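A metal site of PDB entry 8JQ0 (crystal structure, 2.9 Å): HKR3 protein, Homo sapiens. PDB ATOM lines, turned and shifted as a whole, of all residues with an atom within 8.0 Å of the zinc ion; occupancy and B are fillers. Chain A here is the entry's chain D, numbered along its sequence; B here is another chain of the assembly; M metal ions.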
ATOM      1  N   GLU A  32      30.624   9.700  -7.652  1.00  0.00           N
ATOM      2  CA  GLU A  32      30.386   9.013  -6.394  1.00  0.00           C
ATOM      3  C   GLU A  32      30.811   9.903  -5.229  1.00  0.00           C
ATOM      4  O   GLU A  32      31.882  10.505  -5.259  1.00  0.00           O
ATOM      5  CB  GLU A  32      31.150   7.690  -6.352  1.00  0.00           C
ATOM      6  CG  GLU A  32      31.299   7.089  -4.952  1.00  0.00           C
ATOM      7  CD  GLU A  32      31.921   5.706  -4.973  1.00  0.00           C
ATOM      8  OE1 GLU A  32      32.764   5.440  -5.852  1.00  0.00           O
ATOM      9  OE2 GLU A  32      31.574   4.892  -4.091  1.00  0.00           O
ATOM     10  N   CYS A  33      29.959   9.967  -4.202  1.00  0.00           N
ATOM     11  CA  CYS A  33      30.288  10.756  -3.022  1.00  0.00           C
ATOM     12  C   CYS A  33      31.367  10.076  -2.205  1.00  0.00           C
ATOM     13  O   CYS A  33      31.376   8.846  -2.046  1.00  0.00           O
ATOM     14  CB  CYS A  33      29.034  10.969  -2.172  1.00  0.00           C
ATOM     15  SG  CYS A  33      29.388  11.540  -0.496  1.00  0.00           S
ATOM     16  N   THR A  34      32.291  10.873  -1.678  1.00  0.00           N
ATOM     17  CA  THR A  34      33.404  10.334  -0.900  1.00  0.00           C
ATOM     18  C   THR A  34      32.999   9.929   0.517  1.00  0.00           C
ATOM     19  O   THR A  34      33.683   9.108   1.131  1.00  0.00           O
ATOM     20  CB  THR A  34      34.552  11.346  -0.827  1.00  0.00           C
ATOM     21  OG1 THR A  34      34.007  12.658  -0.650  1.00  0.00           O
ATOM     22  CG2 THR A  34      35.371  11.304  -2.102  1.00  0.00           C
ATOM     23  N   GLU A  35      31.900  10.494   1.036  1.00  0.00           N
ATOM     24  CA  GLU A  35      31.469  10.192   2.407  1.00  0.00           C
ATOM     25  C   GLU A  35      30.582   8.941   2.430  1.00  0.00           C
ATOM     26  O   GLU A  35      30.974   7.906   2.956  1.00  0.00           O
ATOM     27  CB  GLU A  35      30.748  11.391   3.014  1.00  0.00           C
ATOM     28  CG  GLU A  35      31.687  12.477   3.540  1.00  0.00           C
ATOM     29  CD  GLU A  35      31.145  13.169   4.771  1.00  0.00           C
ATOM     30  OE1 GLU A  35      30.581  12.468   5.646  1.00  0.00           O
ATOM     31  OE2 GLU A  35      31.279  14.406   4.881  1.00  0.00           O
ATOM     32  N   CYS A  36      29.379   9.049   1.865  1.00  0.00           N
ATOM     33  CA  CYS A  36      28.385   7.988   1.946  1.00  0.00           C
ATOM     34  C   CYS A  36      28.360   7.075   0.725  1.00  0.00           C
ATOM     35  O   CYS A  36      27.535   6.162   0.676  1.00  0.00           O
ATOM     36  CB  CYS A  36      26.992   8.599   2.172  1.00  0.00           C
ATOM     37  SG  CYS A  36      26.266   9.378   0.713  1.00  0.00           S
ATOM     38  N   GLY A  37      29.239   7.306  -0.253  1.00  0.00           N
ATOM     39  CA  GLY A  37      29.326   6.413  -1.399  1.00  0.00           C
ATOM     40  C   GLY A  37      28.201   6.525  -2.402  1.00  0.00           C
ATOM     41  O   GLY A  37      28.102   5.673  -3.285  1.00  0.00           O
ATOM     42  N   TYR A  38      27.351   7.538  -2.282  1.00  0.00           N
ATOM     43  CA  TYR A  38      26.269   7.725  -3.247  1.00  0.00           C
ATOM     44  C   TYR A  38      26.842   8.181  -4.589  1.00  0.00           C
ATOM     45  O   TYR A  38      27.675   9.088  -4.644  1.00  0.00           O
ATOM     46  CB  TYR A  38      25.265   8.752  -2.716  1.00  0.00           C
ATOM     47  CG  TYR A  38      23.870   8.637  -3.293  1.00  0.00           C
ATOM     48  CD1 TYR A  38      23.651   8.746  -4.670  1.00  0.00           C
ATOM     49  CD2 TYR A  38      22.769   8.430  -2.470  1.00  0.00           C
ATOM     50  CE1 TYR A  38      22.380   8.651  -5.193  1.00  0.00           C
ATOM     51  CE2 TYR A  38      21.495   8.329  -2.999  1.00  0.00           C
ATOM     52  CZ  TYR A  38      21.306   8.435  -4.359  1.00  0.00           C
ATOM     53  OH  TYR A  38      20.044   8.339  -4.886  1.00  0.00           O
ATOM     54  N   LYS A  39      26.393   7.539  -5.661  1.00  0.00           N
ATOM     55  CA  LYS A  39      26.829   7.862  -7.025  1.00  0.00           C
ATOM     56  C   LYS A  39      25.713   8.619  -7.737  1.00  0.00           C
ATOM     57  O   LYS A  39      24.571   8.165  -7.761  1.00  0.00           O
ATOM     58  CB  LYS A  39      27.200   6.589  -7.790  1.00  0.00           C
ATOM     59  CG  LYS A  39      28.151   5.677  -7.035  1.00  0.00           C
ATOM     60  CD  LYS A  39      27.923   4.211  -7.379  1.00  0.00           C
ATOM     61  CE  LYS A  39      29.237   3.476  -7.545  1.00  0.00           C
ATOM     62  NZ  LYS A  39      29.024   2.012  -7.733  1.00  0.00           N
ATOM     63  N   PHE A  40      26.066   9.766  -8.326  1.00  0.00           N
ATOM     64  CA  PHE A  40      25.100  10.675  -8.919  1.00  0.00           C
ATOM     65  C   PHE A  40      25.310  10.781 -10.418  1.00  0.00           C
ATOM     66  O   PHE A  40      26.384  10.459 -10.945  1.00  0.00           O
ATOM     67  CB  PHE A  40      25.179  12.066  -8.288  1.00  0.00           C
ATOM     68  CG  PHE A  40      25.016  12.077  -6.796  1.00  0.00           C
ATOM     69  CD1 PHE A  40      23.823  12.505  -6.226  1.00  0.00           C
ATOM     70  CD2 PHE A  40      26.042  11.670  -5.956  1.00  0.00           C
ATOM     71  CE1 PHE A  40      23.659  12.519  -4.857  1.00  0.00           C
ATOM     72  CE2 PHE A  40      25.887  11.683  -4.592  1.00  0.00           C
ATOM     73  CZ  PHE A  40      24.694  12.105  -4.046  1.00  0.00           C
ATOM     74  N   LEU A  46      26.052  16.216  -6.811  1.00  0.00           N
ATOM     75  CA  LEU A  46      26.995  15.901  -5.752  1.00  0.00           C
ATOM     76  C   LEU A  46      27.262  17.126  -4.880  1.00  0.00           C
ATOM     77  O   LEU A  46      27.273  17.041  -3.648  1.00  0.00           O
ATOM     78  CB  LEU A  46      28.299  15.353  -6.331  1.00  0.00           C
ATOM     79  CG  LEU A  46      29.293  14.718  -5.365  1.00  0.00           C
ATOM     80  CD1 LEU A  46      28.585  13.942  -4.265  1.00  0.00           C
ATOM     81  CD2 LEU A  46      30.258  13.812  -6.120  1.00  0.00           C
ATOM     82  N   HIS A  49      24.448  17.633  -2.822  1.00  0.00           N
ATOM     83  CA  HIS A  49      24.323  16.583  -1.811  1.00  0.00           C
ATOM     84  C   HIS A  49      25.284  16.796  -0.648  1.00  0.00           C
ATOM     85  O   HIS A  49      24.913  16.572   0.507  1.00  0.00           O
ATOM     86  CB  HIS A  49      24.556  15.216  -2.456  1.00  0.00           C
ATOM     87  CG  HIS A  49      24.863  14.119  -1.478  1.00  0.00           C
ATOM     88  ND1 HIS A  49      23.877  13.406  -0.832  1.00  0.00           N
ATOM     89  CD2 HIS A  49      26.042  13.619  -1.045  1.00  0.00           C
ATOM     90  CE1 HIS A  49      24.438  12.504  -0.043  1.00  0.00           C
ATOM     91  NE2 HIS A  49      25.756  12.617  -0.153  1.00  0.00           N
ATOM     92  N   MET A  50      26.512  17.224  -0.942  1.00  0.00           N
ATOM     93  CA  MET A  50      27.501  17.423   0.114  1.00  0.00           C
ATOM     94  C   MET A  50      27.137  18.564   1.055  1.00  0.00           C
ATOM     95  O   MET A  50      27.670  18.627   2.161  1.00  0.00           O
ATOM     96  CB  MET A  50      28.887  17.664  -0.493  1.00  0.00           C
ATOM     97  CG  MET A  50      29.419  16.488  -1.301  1.00  0.00           C
ATOM     98  SD  MET A  50      30.143  15.208  -0.254  1.00  0.00           S
ATOM     99  CE  MET A  50      31.405  14.554  -1.354  1.00  0.00           C
ATOM    100  N   ILE A  52      24.333  18.815   2.506  1.00  0.00           N
ATOM    101  CA  ILE A  52      23.571  18.199   3.591  1.00  0.00           C
ATOM    102  C   ILE A  52      24.518  17.524   4.576  1.00  0.00           C
ATOM    103  O   ILE A  52      24.275  17.532   5.794  1.00  0.00           O
ATOM    104  CB  ILE A  52      22.522  17.220   3.026  1.00  0.00           C
ATOM    105  CG1 ILE A  52      21.232  17.959   2.662  1.00  0.00           C
ATOM    106  CG2 ILE A  52      22.209  16.118   4.017  1.00  0.00           C
ATOM    107  CD1 ILE A  52      21.340  18.907   1.475  1.00  0.00           C
ATOM    108  N   HIS A  53      25.606  16.937   4.084  1.00  0.00           N
ATOM    109  CA  HIS A  53      26.590  16.312   4.954  1.00  0.00           C
ATOM    110  C   HIS A  53      27.161  17.310   5.966  1.00  0.00           C
ATOM    111  O   HIS A  53      27.476  16.932   7.101  1.00  0.00           O
ATOM    112  CB  HIS A  53      27.728  15.694   4.136  1.00  0.00           C
ATOM    113  CG  HIS A  53      27.440  14.298   3.676  1.00  0.00           C
ATOM    114  ND1 HIS A  53      27.155  13.268   4.550  1.00  0.00           N
ATOM    115  CD2 HIS A  53      27.417  13.754   2.441  1.00  0.00           C
ATOM    116  CE1 HIS A  53      26.958  12.162   3.869  1.00  0.00           C
ATOM    117  NE2 HIS A  53      27.109  12.423   2.590  1.00  0.00           N
ATOM    118  N   TYR A  59      24.750  10.567   7.613  1.00  0.00           N
ATOM    119  CA  TYR A  59      23.871  10.604   6.457  1.00  0.00           C
ATOM    120  C   TYR A  59      24.325   9.558   5.435  1.00  0.00           C
ATOM    121  O   TYR A  59      25.469   9.598   4.972  1.00  0.00           O
ATOM    122  CB  TYR A  59      23.868  11.993   5.830  1.00  0.00           C
ATOM    123  CG  TYR A  59      22.830  12.173   4.745  1.00  0.00           C
ATOM    124  CD1 TYR A  59      21.543  11.688   4.915  1.00  0.00           C
ATOM    125  CD2 TYR A  59      23.139  12.805   3.553  1.00  0.00           C
ATOM    126  CE1 TYR A  59      20.580  11.840   3.926  1.00  0.00           C
ATOM    127  CE2 TYR A  59      22.194  12.956   2.556  1.00  0.00           C
ATOM    128  CZ  TYR A  59      20.916  12.477   2.746  1.00  0.00           C
ATOM    129  OH  TYR A  59      19.977  12.628   1.762  1.00  0.00           O
ATOM    130  N   ASN A  60      23.420   8.650   5.088  1.00  0.00           N
ATOM    131  CA  ASN A  60      23.696   7.615   4.083  1.00  0.00           C
ATOM    132  C   ASN A  60      22.402   7.235   3.394  1.00  0.00           C
ATOM    133  O   ASN A  60      21.824   6.173   3.646  1.00  0.00           O
ATOM    134  CB  ASN A  60      24.356   6.398   4.736  1.00  0.00           C
ATOM    135  CG  ASN A  60      25.402   5.752   3.840  1.00  0.00           C
ATOM    136  OD1 ASN A  60      25.338   5.862   2.611  1.00  0.00           O
ATOM    137  ND2 ASN A  60      26.374   5.084   4.443  1.00  0.00           N
ATOM    138  N   PRO A  61      21.903   8.100   2.505  1.00  0.00           N
ATOM    139  CA  PRO A  61      20.617   7.818   1.848  1.00  0.00           C
ATOM    140  C   PRO A  61      20.764   6.691   0.835  1.00  0.00           C
ATOM    141  O   PRO A  61      21.770   6.575   0.132  1.00  0.00           O
ATOM    142  CB  PRO A  61      20.279   9.144   1.166  1.00  0.00           C
ATOM    143  CG  PRO A  61      21.610   9.764   0.882  1.00  0.00           C
ATOM    144  CD  PRO A  61      22.494   9.364   2.041  1.00  0.00           C
ATOM    145  P    DA B   9      20.583  14.116  -2.039  1.00  0.00           P
ATOM    146  OP1  DA B   9      21.484  13.423  -1.104  1.00  0.00           O
ATOM    147  OP2  DA B   9      20.801  15.548  -2.351  1.00  0.00           O
ATOM    148  O5'  DA B   9      20.548  13.306  -3.420  1.00  0.00           O
ATOM    149  C5'  DA B   9      20.293  11.912  -3.415  1.00  0.00           C
ATOM    150  C4'  DA B   9      19.281  11.537  -4.478  1.00  0.00           C
ATOM    151  O4'  DA B   9      18.137  12.420  -4.411  1.00  0.00           O
ATOM    152  C3'  DA B   9      19.790  11.617  -5.918  1.00  0.00           C
ATOM    153  O3'  DA B   9      19.275  10.532  -6.673  1.00  0.00           O
ATOM    154  C2'  DA B   9      19.231  12.952  -6.408  1.00  0.00           C
ATOM    155  C1'  DA B   9      17.902  12.981  -5.682  1.00  0.00           C
ATOM    156  N9   DA B   9      17.371  14.327  -5.501  1.00  0.00           N
ATOM    157  C8   DA B   9      17.918  15.340  -4.764  1.00  0.00           C
ATOM    158  N7   DA B   9      17.222  16.452  -4.778  1.00  0.00           N
ATOM    159  C5   DA B   9      16.140  16.147  -5.589  1.00  0.00           C
ATOM    160  C6   DA B   9      15.034  16.911  -6.010  1.00  0.00           C
ATOM    161  N6   DA B   9      14.833  18.183  -5.648  1.00  0.00           N
ATOM    162  N1   DA B   9      14.127  16.304  -6.814  1.00  0.00           N
ATOM    163  C2   DA B   9      14.337  15.032  -7.180  1.00  0.00           C
ATOM    164  N3   DA B   9      15.338  14.219  -6.839  1.00  0.00           N
ATOM    165  C4   DA B   9      16.211  14.849  -6.042  1.00  0.00           C
HETATM  166 ZN    ZN M   1      27.377  11.446   0.607  1.00  0.00          ZN
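O of Tyr 38 is in hydrogen-bond range of N of Cys 33 (2.5 Å). The side-chain sulfur of Cys 33 sits close to the side-chain sulfur of Met 50, at 3.8 Å. SG of Cys 33 lies close to N of Glu 35. OP1 of DA 9 of chain B sits at hydrogen-bond distance from ND1 of His 49 (2.4 Å). OD1 of Asn 60 sits close to O of Cys 36, at 2.9 Å. N of Tyr 38 lies close to SG of Cys 36 (3.7 Å).
NE2 of His 49 binds the zinc ion. The zinc ion is bound by NE2 of His 53 (2.2 Å). SG of Cys 33 is bound to the zinc ion. SG of Cys 36 is bound to the zinc ion (2.3 Å). The zinc ion has four donor atoms within binding distance.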
